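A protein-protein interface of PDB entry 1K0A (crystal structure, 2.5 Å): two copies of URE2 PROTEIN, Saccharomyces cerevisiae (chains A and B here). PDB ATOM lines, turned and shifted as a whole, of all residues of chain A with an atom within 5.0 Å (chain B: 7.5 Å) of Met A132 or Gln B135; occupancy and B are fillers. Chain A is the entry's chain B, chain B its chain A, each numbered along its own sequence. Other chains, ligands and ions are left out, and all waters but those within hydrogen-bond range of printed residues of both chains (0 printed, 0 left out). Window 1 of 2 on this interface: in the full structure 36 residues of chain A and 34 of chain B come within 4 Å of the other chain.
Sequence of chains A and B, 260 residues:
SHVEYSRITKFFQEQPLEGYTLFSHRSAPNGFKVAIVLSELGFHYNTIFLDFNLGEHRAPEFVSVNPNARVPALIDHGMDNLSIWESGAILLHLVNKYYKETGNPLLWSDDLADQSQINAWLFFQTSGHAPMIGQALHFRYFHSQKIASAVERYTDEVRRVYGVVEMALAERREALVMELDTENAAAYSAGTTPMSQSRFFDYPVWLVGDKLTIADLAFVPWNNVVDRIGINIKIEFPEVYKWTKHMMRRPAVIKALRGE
Met A132 touches Gln B135, but with the chains exchanged Gln A135 does not touch Met B132 (4.8 Å). Gln A135 touches Arg B153, and with the chains exchanged Arg A153 touches Gln B135. Gln A135 touches Tyr B154, and with the chains exchanged Tyr A154 touches Gln B135. Tyr A154 touches its own counterpart, Tyr B154.
Among the printed residues, merely in contact across the chains: Met A132 with Gln B135 (3.5 Å), Arg A153 with Phe B139 (3.9 Å) and Tyr A154 with Phe B139 (3.2 Å).
NE2 of Gln B135 lies close to NH2 of Arg A153, 2.7 Å away. NE2 of Gln B135 sits at hydrogen-bond distance from OH of Tyr A154 (2.6 Å). NH1 of Arg A153 sits close to NE2 of His B138, at 3.3 Å. NH2 of Arg B153 lies close to NE2 of Gln A135 (3.2 Å). The side-chain hydroxyl of Tyr B154 sits at hydrogen-bond distance from the side-chain amide nitrogen of Gln A135 (2.7 Å). The side-chain hydroxyl of Tyr A154 is in hydrogen-bond range of the side-chain hydroxyl of Tyr B154 (3.2 Å).
Met A132 touches one residue of chain B. Of the printed residues of chain B, Arg A153 touches Gln B135 (2.7 Å), His B138 (3.2 Å) and Phe B139 (3.9 Å). Printed residues of chain B within 4 Å of Tyr A154: Gln B135, Phe B139 and Tyr B154. Gln B135 touches three residues of chain A. Printed residues of chain A within 4 Å of Phe B139: Arg A153 (3.9 Å) and Tyr A154 (3.2 Å). Printed residues of chain A within 4 Å of Arg B153: Gln A135. Of the printed residues of chain A, Tyr B154 touches Gln A135 and Tyr A154. The nearest residue of chain B that does not touch Met A132 is Pro B131 (5.4 Å). The nearest printed residue of chain A that does not touch Gln B135 is Gln A135 (5.4 Å).
The backbone carbonyl oxygen (O) of His B138 is in hydrogen-bond range of the backbone NH (N) of His B143 (2.8 Å). The backbone carbonyl oxygen (O) of Pro A131 sits close to the side-chain amide oxygen (OE1) of Gln A135 (3.2 Å). The guanidinium group (NE) of Arg A153 is in hydrogen-bond range of the side-chain hydroxyl (OH) of Tyr A154 (3.5 Å).
Of the 13 printed residues of chain A, 4 touch a printed residue of chain B. Hydrophobic or aromatic side chains of chain A within 4 Å of the printed part of chain B: Met A132 and Tyr A154. Of the 22 printed residues of chain B, 5 touch a printed residue of chain A. Among the printed residues, 9 pairs touch across the chains. Among the printed residues, no Asp or Glu carboxylate lies within 4 Å of a Lys or Arg side-chain nitrogen of the other chain.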
ATOM      1  N   GLY A 128       4.110   2.720 -20.515  1.00  0.00           N
ATOM      2  CA  GLY A 128       4.829   3.065 -21.727  1.00  0.00           C
ATOM      3  C   GLY A 128       5.509   4.411 -21.692  1.00  0.00           C
ATOM      4  O   GLY A 128       6.100   4.829 -22.674  1.00  0.00           O
ATOM      5  N   HIS A 129       5.448   5.085 -20.555  1.00  0.00           N
ATOM      6  CA  HIS A 129       6.054   6.405 -20.423  1.00  0.00           C
ATOM      7  C   HIS A 129       7.028   6.382 -19.256  1.00  0.00           C
ATOM      8  O   HIS A 129       8.235   6.486 -19.438  1.00  0.00           O
ATOM      9  CB  HIS A 129       4.939   7.438 -20.205  1.00  0.00           C
ATOM     10  CG  HIS A 129       5.413   8.853 -20.097  1.00  0.00           C
ATOM     11  ND1 HIS A 129       5.384   9.557 -18.910  1.00  0.00           N
ATOM     12  CD2 HIS A 129       5.850   9.722 -21.039  1.00  0.00           C
ATOM     13  CE1 HIS A 129       5.775  10.799 -19.128  1.00  0.00           C
ATOM     14  NE2 HIS A 129       6.064  10.926 -20.412  1.00  0.00           N
ATOM     15  N   ALA A 130       6.500   6.221 -18.054  1.00  0.00           N
ATOM     16  CA  ALA A 130       7.344   6.178 -16.868  1.00  0.00           C
ATOM     17  C   ALA A 130       8.496   5.160 -16.965  1.00  0.00           C
ATOM     18  O   ALA A 130       9.629   5.479 -16.623  1.00  0.00           O
ATOM     19  CB  ALA A 130       6.488   5.894 -15.622  1.00  0.00           C
ATOM     20  N   PRO A 131       8.221   3.922 -17.420  1.00  0.00           N
ATOM     21  CA  PRO A 131       9.319   2.952 -17.508  1.00  0.00           C
ATOM     22  C   PRO A 131      10.397   3.366 -18.522  1.00  0.00           C
ATOM     23  O   PRO A 131      11.599   3.294 -18.250  1.00  0.00           O
ATOM     24  CB  PRO A 131       8.610   1.665 -17.922  1.00  0.00           C
ATOM     25  CG  PRO A 131       7.205   1.859 -17.409  1.00  0.00           C
ATOM     26  CD  PRO A 131       6.935   3.287 -17.759  1.00  0.00           C
ATOM     27  N   MET A 132       9.955   3.804 -19.694  1.00  0.00           N
ATOM     28  CA  MET A 132      10.878   4.216 -20.735  1.00  0.00           C
ATOM     29  C   MET A 132      11.716   5.403 -20.263  1.00  0.00           C
ATOM     30  O   MET A 132      12.933   5.431 -20.483  1.00  0.00           O
ATOM     31  CB  MET A 132      10.102   4.538 -22.008  1.00  0.00           C
ATOM     32  CG  MET A 132       9.221   3.365 -22.492  1.00  0.00           C
ATOM     33  SD  MET A 132      10.148   1.921 -23.136  1.00  0.00           S
ATOM     34  CE  MET A 132      10.524   1.005 -21.606  1.00  0.00           C
ATOM     35  N   ILE A 133      11.084   6.377 -19.602  1.00  0.00           N
ATOM     36  CA  ILE A 133      11.840   7.517 -19.086  1.00  0.00           C
ATOM     37  C   ILE A 133      12.845   6.976 -18.080  1.00  0.00           C
ATOM     38  O   ILE A 133      13.994   7.398 -18.053  1.00  0.00           O
ATOM     39  CB  ILE A 133      10.945   8.541 -18.376  1.00  0.00           C
ATOM     40  CG1 ILE A 133      10.124   9.311 -19.412  1.00  0.00           C
ATOM     41  CG2 ILE A 133      11.803   9.510 -17.551  1.00  0.00           C
ATOM     42  CD1 ILE A 133       9.067  10.206 -18.813  1.00  0.00           C
ATOM     43  N   GLY A 134      12.403   6.028 -17.267  1.00  0.00           N
ATOM     44  CA  GLY A 134      13.274   5.429 -16.276  1.00  0.00           C
ATOM     45  C   GLY A 134      14.472   4.700 -16.860  1.00  0.00           C
ATOM     46  O   GLY A 134      15.540   4.690 -16.259  1.00  0.00           O
ATOM     47  N   GLN A 135      14.308   4.093 -18.035  1.00  0.00           N
ATOM     48  CA  GLN A 135      15.403   3.364 -18.671  1.00  0.00           C
ATOM     49  C   GLN A 135      16.388   4.312 -19.348  1.00  0.00           C
ATOM     50  O   GLN A 135      17.582   4.022 -19.427  1.00  0.00           O
ATOM     51  CB  GLN A 135      14.864   2.358 -19.688  1.00  0.00           C
ATOM     52  CG  GLN A 135      13.812   1.410 -19.122  1.00  0.00           C
ATOM     53  CD  GLN A 135      14.163   0.898 -17.739  1.00  0.00           C
ATOM     54  OE1 GLN A 135      13.537   1.277 -16.750  1.00  0.00           O
ATOM     55  NE2 GLN A 135      15.165   0.037 -17.659  1.00  0.00           N
ATOM     56  N   ALA A 136      15.887   5.440 -19.839  1.00  0.00           N
ATOM     57  CA  ALA A 136      16.744   6.424 -20.477  1.00  0.00           C
ATOM     58  C   ALA A 136      17.645   6.991 -19.398  1.00  0.00           C
ATOM     59  O   ALA A 136      18.841   7.172 -19.603  1.00  0.00           O
ATOM     60  CB  ALA A 136      15.915   7.537 -21.108  1.00  0.00           C
ATOM     61  N   ARG A 153      17.700   4.392 -27.746  1.00  0.00           N
ATOM     62  CA  ARG A 153      16.509   3.555 -27.812  1.00  0.00           C
ATOM     63  C   ARG A 153      15.356   4.101 -26.974  1.00  0.00           C
ATOM     64  O   ARG A 153      14.251   4.287 -27.490  1.00  0.00           O
ATOM     65  CB  ARG A 153      16.818   2.126 -27.359  1.00  0.00           C
ATOM     66  CG  ARG A 153      15.559   1.252 -27.078  1.00  0.00           C
ATOM     67  CD  ARG A 153      15.974  -0.100 -26.506  1.00  0.00           C
ATOM     68  NE  ARG A 153      14.876  -0.955 -26.068  1.00  0.00           N
ATOM     69  CZ  ARG A 153      13.965  -1.490 -26.876  1.00  0.00           C
ATOM     70  NH1 ARG A 153      14.007  -1.257 -28.182  1.00  0.00           N
ATOM     71  NH2 ARG A 153      13.020  -2.278 -26.378  1.00  0.00           N
ATOM     72  N   TYR A 154      15.619   4.350 -25.691  1.00  0.00           N
ATOM     73  CA  TYR A 154      14.602   4.856 -24.778  1.00  0.00           C
ATOM     74  C   TYR A 154      14.291   6.338 -24.927  1.00  0.00           C
ATOM     75  O   TYR A 154      13.150   6.746 -24.728  1.00  0.00           O
ATOM     76  CB  TYR A 154      14.983   4.549 -23.327  1.00  0.00           C
ATOM     77  CG  TYR A 154      15.083   3.067 -23.068  1.00  0.00           C
ATOM     78  CD1 TYR A 154      16.326   2.443 -22.970  1.00  0.00           C
ATOM     79  CD2 TYR A 154      13.935   2.272 -23.000  1.00  0.00           C
ATOM     80  CE1 TYR A 154      16.429   1.068 -22.817  1.00  0.00           C
ATOM     81  CE2 TYR A 154      14.025   0.879 -22.851  1.00  0.00           C
ATOM     82  CZ  TYR A 154      15.279   0.286 -22.760  1.00  0.00           C
ATOM     83  OH  TYR A 154      15.404  -1.081 -22.627  1.00  0.00           O
ATOM     84  N   GLU A 157      11.848   6.496 -27.757  1.00  0.00           N
ATOM     85  CA  GLU A 157      10.541   5.994 -27.387  1.00  0.00           C
ATOM     86  C   GLU A 157       9.820   7.005 -26.512  1.00  0.00           C
ATOM     87  O   GLU A 157       8.605   7.174 -26.637  1.00  0.00           O
ATOM     88  CB  GLU A 157      10.662   4.643 -26.671  1.00  0.00           C
ATOM     89  CG  GLU A 157       9.317   3.967 -26.374  1.00  0.00           C
ATOM     90  CD  GLU A 157       8.501   3.661 -27.635  1.00  0.00           C
ATOM     91  OE1 GLU A 157       7.345   3.214 -27.503  1.00  0.00           O
ATOM     92  OE2 GLU A 157       9.004   3.858 -28.760  1.00  0.00           O
ATOM     93  N   VAL A 158      10.557   7.690 -25.638  1.00  0.00           N
ATOM     94  CA  VAL A 158       9.932   8.701 -24.787  1.00  0.00           C
ATOM     95  C   VAL A 158       9.431   9.840 -25.673  1.00  0.00           C
ATOM     96  O   VAL A 158       8.394  10.453 -25.384  1.00  0.00           O
ATOM     97  CB  VAL A 158      10.900   9.289 -23.741  1.00  0.00           C
ATOM     98  CG1 VAL A 158      10.294  10.547 -23.136  1.00  0.00           C
ATOM     99  CG2 VAL A 158      11.166   8.275 -22.632  1.00  0.00           C
ATOM    100  N   HIS B 129       6.178  -6.345 -15.050  1.00  0.00           N
ATOM    101  CA  HIS B 129       6.482  -7.681 -15.542  1.00  0.00           C
ATOM    102  C   HIS B 129       6.688  -7.648 -17.058  1.00  0.00           C
ATOM    103  O   HIS B 129       7.791  -7.870 -17.554  1.00  0.00           O
ATOM    104  CB  HIS B 129       5.325  -8.606 -15.152  1.00  0.00           C
ATOM    105  CG  HIS B 129       5.466 -10.014 -15.635  1.00  0.00           C
ATOM    106  ND1 HIS B 129       4.528 -10.614 -16.447  1.00  0.00           N
ATOM    107  CD2 HIS B 129       6.399 -10.960 -15.375  1.00  0.00           C
ATOM    108  CE1 HIS B 129       4.875 -11.870 -16.665  1.00  0.00           C
ATOM    109  NE2 HIS B 129       6.006 -12.105 -16.025  1.00  0.00           N
ATOM    110  N   ALA B 130       5.627  -7.328 -17.786  1.00  0.00           N
ATOM    111  CA  ALA B 130       5.659  -7.272 -19.246  1.00  0.00           C
ATOM    112  C   ALA B 130       6.766  -6.426 -19.865  1.00  0.00           C
ATOM    113  O   ALA B 130       7.495  -6.886 -20.740  1.00  0.00           O
ATOM    114  CB  ALA B 130       4.303  -6.798 -19.776  1.00  0.00           C
ATOM    115  N   PRO B 131       6.899  -5.170 -19.430  1.00  0.00           N
ATOM    116  CA  PRO B 131       7.945  -4.324 -20.007  1.00  0.00           C
ATOM    117  C   PRO B 131       9.346  -4.868 -19.775  1.00  0.00           C
ATOM    118  O   PRO B 131      10.197  -4.820 -20.665  1.00  0.00           O
ATOM    119  CB  PRO B 131       7.731  -2.979 -19.309  1.00  0.00           C
ATOM    120  CG  PRO B 131       6.267  -3.019 -18.903  1.00  0.00           C
ATOM    121  CD  PRO B 131       6.117  -4.432 -18.424  1.00  0.00           C
ATOM    122  N   MET B 132       9.591  -5.391 -18.579  1.00  0.00           N
ATOM    123  CA  MET B 132      10.916  -5.919 -18.278  1.00  0.00           C
ATOM    124  C   MET B 132      11.222  -7.139 -19.132  1.00  0.00           C
ATOM    125  O   MET B 132      12.351  -7.304 -19.609  1.00  0.00           O
ATOM    126  CB  MET B 132      11.045  -6.246 -16.787  1.00  0.00           C
ATOM    127  CG  MET B 132      10.926  -4.996 -15.901  1.00  0.00           C
ATOM    128  SD  MET B 132      11.933  -3.567 -16.465  1.00  0.00           S
ATOM    129  CE  MET B 132      12.893  -3.173 -14.974  1.00  0.00           C
ATOM    130  N   ILE B 133      10.222  -7.989 -19.338  1.00  0.00           N
ATOM    131  CA  ILE B 133      10.425  -9.163 -20.164  1.00  0.00           C
ATOM    132  C   ILE B 133      10.718  -8.690 -21.580  1.00  0.00           C
ATOM    133  O   ILE B 133      11.606  -9.210 -22.246  1.00  0.00           O
ATOM    134  CB  ILE B 133       9.179 -10.067 -20.160  1.00  0.00           C
ATOM    135  CG1 ILE B 133       8.915 -10.569 -18.737  1.00  0.00           C
ATOM    136  CG2 ILE B 133       9.378 -11.240 -21.106  1.00  0.00           C
ATOM    137  CD1 ILE B 133       7.689 -11.431 -18.614  1.00  0.00           C
ATOM    138  N   GLY B 134       9.982  -7.679 -22.027  1.00  0.00           N
ATOM    139  CA  GLY B 134      10.187  -7.161 -23.364  1.00  0.00           C
ATOM    140  C   GLY B 134      11.571  -6.572 -23.598  1.00  0.00           C
ATOM    141  O   GLY B 134      12.103  -6.646 -24.703  1.00  0.00           O
ATOM    142  N   GLN B 135      12.161  -5.973 -22.571  1.00  0.00           N
ATOM    143  CA  GLN B 135      13.486  -5.387 -22.736  1.00  0.00           C
ATOM    144  C   GLN B 135      14.545  -6.479 -22.755  1.00  0.00           C
ATOM    145  O   GLN B 135      15.560  -6.362 -23.444  1.00  0.00           O
ATOM    146  CB  GLN B 135      13.768  -4.371 -21.626  1.00  0.00           C
ATOM    147  CG  GLN B 135      12.747  -3.248 -21.602  1.00  0.00           C
ATOM    148  CD  GLN B 135      12.611  -2.548 -22.950  1.00  0.00           C
ATOM    149  OE1 GLN B 135      11.582  -1.947 -23.241  1.00  0.00           O
ATOM    150  NE2 GLN B 135      13.655  -2.614 -23.771  1.00  0.00           N
ATOM    151  N   ALA B 136      14.299  -7.547 -22.009  1.00  0.00           N
ATOM    152  CA  ALA B 136      15.233  -8.653 -21.976  1.00  0.00           C
ATOM    153  C   ALA B 136      15.270  -9.278 -23.372  1.00  0.00           C
ATOM    154  O   ALA B 136      16.346  -9.564 -23.897  1.00  0.00           O
ATOM    155  CB  ALA B 136      14.801  -9.685 -20.931  1.00  0.00           C
ATOM    156  N   LEU B 137      14.101  -9.478 -23.979  1.00  0.00           N
ATOM    157  CA  LEU B 137      14.057 -10.067 -25.313  1.00  0.00           C
ATOM    158  C   LEU B 137      14.729  -9.154 -26.316  1.00  0.00           C
ATOM    159  O   LEU B 137      15.480  -9.610 -27.172  1.00  0.00           O
ATOM    160  CB  LEU B 137      12.620 -10.323 -25.764  1.00  0.00           C
ATOM    161  CG  LEU B 137      11.854 -11.465 -25.103  1.00  0.00           C
ATOM    162  CD1 LEU B 137      10.396 -11.459 -25.563  1.00  0.00           C
ATOM    163  CD2 LEU B 137      12.519 -12.780 -25.452  1.00  0.00           C
ATOM    164  N   HIS B 138      14.469  -7.858 -26.207  1.00  0.00           N
ATOM    165  CA  HIS B 138      15.059  -6.921 -27.143  1.00  0.00           C
ATOM    166  C   HIS B 138      16.585  -6.943 -27.184  1.00  0.00           C
ATOM    167  O   HIS B 138      17.181  -6.998 -28.260  1.00  0.00           O
ATOM    168  CB  HIS B 138      14.621  -5.492 -26.846  1.00  0.00           C
ATOM    169  CG  HIS B 138      15.323  -4.483 -27.696  1.00  0.00           C
ATOM    170  ND1 HIS B 138      15.066  -4.345 -29.043  1.00  0.00           N
ATOM    171  CD2 HIS B 138      16.358  -3.652 -27.422  1.00  0.00           C
ATOM    172  CE1 HIS B 138      15.914  -3.475 -29.563  1.00  0.00           C
ATOM    173  NE2 HIS B 138      16.709  -3.041 -28.601  1.00  0.00           N
ATOM    174  N   PHE B 139      17.217  -6.866 -26.017  1.00  0.00           N
ATOM    175  CA  PHE B 139      18.669  -6.847 -25.959  1.00  0.00           C
ATOM    176  C   PHE B 139      19.335  -8.177 -26.249  1.00  0.00           C
ATOM    177  O   PHE B 139      20.422  -8.207 -26.815  1.00  0.00           O
ATOM    178  CB  PHE B 139      19.145  -6.288 -24.616  1.00  0.00           C
ATOM    179  CG  PHE B 139      18.992  -4.800 -24.508  1.00  0.00           C
ATOM    180  CD1 PHE B 139      17.928  -4.240 -23.807  1.00  0.00           C
ATOM    181  CD2 PHE B 139      19.891  -3.951 -25.155  1.00  0.00           C
ATOM    182  CE1 PHE B 139      17.760  -2.860 -23.753  1.00  0.00           C
ATOM    183  CE2 PHE B 139      19.733  -2.573 -25.109  1.00  0.00           C
ATOM    184  CZ  PHE B 139      18.665  -2.023 -24.407  1.00  0.00           C
ATOM    185  N   ARG B 140      18.692  -9.273 -25.877  1.00  0.00           N
ATOM    186  CA  ARG B 140      19.271 -10.568 -26.156  1.00  0.00           C
ATOM    187  C   ARG B 140      19.056 -10.986 -27.613  1.00  0.00           C
ATOM    188  O   ARG B 140      19.778 -11.842 -28.120  1.00  0.00           O
ATOM    189  CB  ARG B 140      18.685 -11.650 -25.239  1.00  0.00           C
ATOM    190  CG  ARG B 140      19.249 -13.030 -25.557  1.00  0.00           C
ATOM    191  CD  ARG B 140      18.812 -14.123 -24.603  1.00  0.00           C
ATOM    192  NE  ARG B 140      19.492 -15.378 -24.927  1.00  0.00           N
ATOM    193  CZ  ARG B 140      19.272 -16.538 -24.315  1.00  0.00           C
ATOM    194  NH1 ARG B 140      19.941 -17.621 -24.685  1.00  0.00           N
ATOM    195  NH2 ARG B 140      18.380 -16.619 -23.333  1.00  0.00           N
ATOM    196  N   TYR B 141      18.088 -10.386 -28.302  1.00  0.00           N
ATOM    197  CA  TYR B 141      17.829 -10.800 -29.676  1.00  0.00           C
ATOM    198  C   TYR B 141      17.724  -9.749 -30.767  1.00  0.00           C
ATOM    199  O   TYR B 141      18.212  -9.965 -31.882  1.00  0.00           O
ATOM    200  CB  TYR B 141      16.549 -11.630 -29.742  1.00  0.00           C
ATOM    201  CG  TYR B 141      16.542 -12.887 -28.909  1.00  0.00           C
ATOM    202  CD1 TYR B 141      15.658 -13.028 -27.832  1.00  0.00           C
ATOM    203  CD2 TYR B 141      17.370 -13.964 -29.235  1.00  0.00           C
ATOM    204  CE1 TYR B 141      15.592 -14.214 -27.109  1.00  0.00           C
ATOM    205  CE2 TYR B 141      17.315 -15.156 -28.515  1.00  0.00           C
ATOM    206  CZ  TYR B 141      16.425 -15.275 -27.458  1.00  0.00           C
ATOM    207  OH  TYR B 141      16.366 -16.458 -26.765  1.00  0.00           O
ATOM    208  N   HIS B 143      18.571  -6.126 -30.505  1.00  0.00           N
ATOM    209  CA  HIS B 143      19.324  -4.874 -30.465  1.00  0.00           C
ATOM    210  C   HIS B 143      20.411  -4.831 -31.537  1.00  0.00           C
ATOM    211  O   HIS B 143      20.986  -5.862 -31.894  1.00  0.00           O
ATOM    212  CB  HIS B 143      19.966  -4.651 -29.099  1.00  0.00           C
ATOM    213  CG  HIS B 143      20.267  -3.213 -28.815  1.00  0.00           C
ATOM    214  ND1 HIS B 143      21.471  -2.788 -28.299  1.00  0.00           N
ATOM    215  CD2 HIS B 143      19.511  -2.101 -28.968  1.00  0.00           C
ATOM    216  CE1 HIS B 143      21.445  -1.476 -28.146  1.00  0.00           C
ATOM    217  NE2 HIS B 143      20.265  -1.034 -28.543  1.00  0.00           N
ATOM    218  N   ALA B 150      23.043  -5.242 -20.226  1.00  0.00           N
ATOM    219  CA  ALA B 150      21.662  -4.807 -20.417  1.00  0.00           C
ATOM    220  C   ALA B 150      20.749  -6.019 -20.345  1.00  0.00           C
ATOM    221  O   ALA B 150      19.672  -5.954 -19.760  1.00  0.00           O
ATOM    222  CB  ALA B 150      21.505  -4.116 -21.765  1.00  0.00           C
ATOM    223  N   VAL B 151      21.195  -7.125 -20.939  1.00  0.00           N
ATOM    224  CA  VAL B 151      20.430  -8.364 -20.949  1.00  0.00           C
ATOM    225  C   VAL B 151      20.311  -8.933 -19.541  1.00  0.00           C
ATOM    226  O   VAL B 151      19.264  -9.461 -19.165  1.00  0.00           O
ATOM    227  CB  VAL B 151      21.097  -9.418 -21.852  1.00  0.00           C
ATOM    228  CG1 VAL B 151      20.347 -10.733 -21.758  1.00  0.00           C
ATOM    229  CG2 VAL B 151      21.120  -8.929 -23.291  1.00  0.00           C
ATOM    230  N   ARG B 153      20.598  -7.164 -16.622  1.00  0.00           N
ATOM    231  CA  ARG B 153      19.804  -6.224 -15.834  1.00  0.00           C
ATOM    232  C   ARG B 153      18.314  -6.565 -15.903  1.00  0.00           C
ATOM    233  O   ARG B 153      17.656  -6.770 -14.879  1.00  0.00           O
ATOM    234  CB  ARG B 153      20.017  -4.804 -16.356  1.00  0.00           C
ATOM    235  CG  ARG B 153      18.969  -3.795 -15.919  1.00  0.00           C
ATOM    236  CD  ARG B 153      19.103  -2.547 -16.772  1.00  0.00           C
ATOM    237  NE  ARG B 153      18.108  -1.526 -16.467  1.00  0.00           N
ATOM    238  CZ  ARG B 153      18.012  -0.900 -15.297  1.00  0.00           C
ATOM    239  NH1 ARG B 153      18.855  -1.194 -14.308  1.00  0.00           N
ATOM    240  NH2 ARG B 153      17.090   0.040 -15.127  1.00  0.00           N
ATOM    241  N   TYR B 154      17.795  -6.628 -17.125  1.00  0.00           N
ATOM    242  CA  TYR B 154      16.393  -6.935 -17.349  1.00  0.00           C
ATOM    243  C   TYR B 154      16.037  -8.389 -17.068  1.00  0.00           C
ATOM    244  O   TYR B 154      14.916  -8.691 -16.671  1.00  0.00           O
ATOM    245  CB  TYR B 154      16.019  -6.554 -18.781  1.00  0.00           C
ATOM    246  CG  TYR B 154      16.168  -5.070 -19.033  1.00  0.00           C
ATOM    247  CD1 TYR B 154      16.980  -4.594 -20.052  1.00  0.00           C
ATOM    248  CD2 TYR B 154      15.504  -4.141 -18.233  1.00  0.00           C
ATOM    249  CE1 TYR B 154      17.130  -3.225 -20.273  1.00  0.00           C
ATOM    250  CE2 TYR B 154      15.649  -2.774 -18.445  1.00  0.00           C
ATOM    251  CZ  TYR B 154      16.461  -2.325 -19.466  1.00  0.00           C
ATOM    252  OH  TYR B 154      16.597  -0.973 -19.684  1.00  0.00           O
ATOM    253  N   THR B 155      16.988  -9.293 -17.270  1.00  0.00           N
ATOM    254  CA  THR B 155      16.742 -10.703 -17.004  1.00  0.00           C
ATOM    255  C   THR B 155      16.633 -10.898 -15.496  1.00  0.00           C
ATOM    256  O   THR B 155      15.827 -11.694 -15.013  1.00  0.00           O
ATOM    257  CB  THR B 155      17.880 -11.590 -17.548  1.00  0.00           C
ATOM    258  OG1 THR B 155      17.967 -11.436 -18.971  1.00  0.00           O
ATOM    259  CG2 THR B 155      17.607 -13.050 -17.223  1.00  0.00           C
ATOM    260  N   VAL B 158      13.259  -9.572 -14.283  1.00  0.00           N
ATOM    261  CA  VAL B 158      12.155 -10.473 -14.565  1.00  0.00           C
ATOM    262  C   VAL B 158      12.140 -11.534 -13.473  1.00  0.00           C
ATOM    263  O   VAL B 158      11.072 -11.949 -13.019  1.00  0.00           O
ATOM    264  CB  VAL B 158      12.303 -11.143 -15.942  1.00  0.00           C
ATOM    265  CG1 VAL B 158      11.207 -12.174 -16.134  1.00  0.00           C
ATOM    266  CG2 VAL B 158      12.223 -10.097 -17.030  1.00  0.00           C
ATOM    267  N   TRP B 222       2.539 -14.202 -20.721  1.00  0.00           N
ATOM    268  CA  TRP B 222       3.952 -13.896 -20.571  1.00  0.00           C
ATOM    269  C   TRP B 222       4.774 -15.040 -19.965  1.00  0.00           C
ATOM    270  O   TRP B 222       5.934 -15.238 -20.337  1.00  0.00           O
ATOM    271  CB  TRP B 222       4.122 -12.609 -19.762  1.00  0.00           C
ATOM    272  CG  TRP B 222       3.579 -11.399 -20.481  1.00  0.00           C
ATOM    273  CD1 TRP B 222       2.304 -10.905 -20.410  1.00  0.00           C
ATOM    274  CD2 TRP B 222       4.277 -10.575 -21.429  1.00  0.00           C
ATOM    275  NE1 TRP B 222       2.167  -9.825 -21.253  1.00  0.00           N
ATOM    276  CE2 TRP B 222       3.361  -9.600 -21.891  1.00  0.00           C
ATOM    277  CE3 TRP B 222       5.587 -10.565 -21.932  1.00  0.00           C
ATOM    278  CZ2 TRP B 222       3.713  -8.622 -22.837  1.00  0.00           C
ATOM    279  CZ3 TRP B 222       5.939  -9.592 -22.870  1.00  0.00           C
ATOM    280  CH2 TRP B 222       5.002  -8.633 -23.312  1.00  0.00           C
ATOM    281  N   ILE B 229      14.354 -16.107 -22.400  1.00  0.00           N
ATOM    282  CA  ILE B 229      15.361 -15.213 -21.852  1.00  0.00           C
ATOM    283  C   ILE B 229      16.103 -15.974 -20.764  1.00  0.00           C
ATOM    284  O   ILE B 229      16.841 -15.395 -19.967  1.00  0.00           O
ATOM    285  CB  ILE B 229      14.768 -13.889 -21.277  1.00  0.00           C
ATOM    286  CG1 ILE B 229      13.670 -14.183 -20.267  1.00  0.00           C
ATOM    287  CG2 ILE B 229      14.260 -13.015 -22.403  1.00  0.00           C
ATOM    288  CD1 ILE B 229      13.157 -12.953 -19.567  1.00  0.00           C
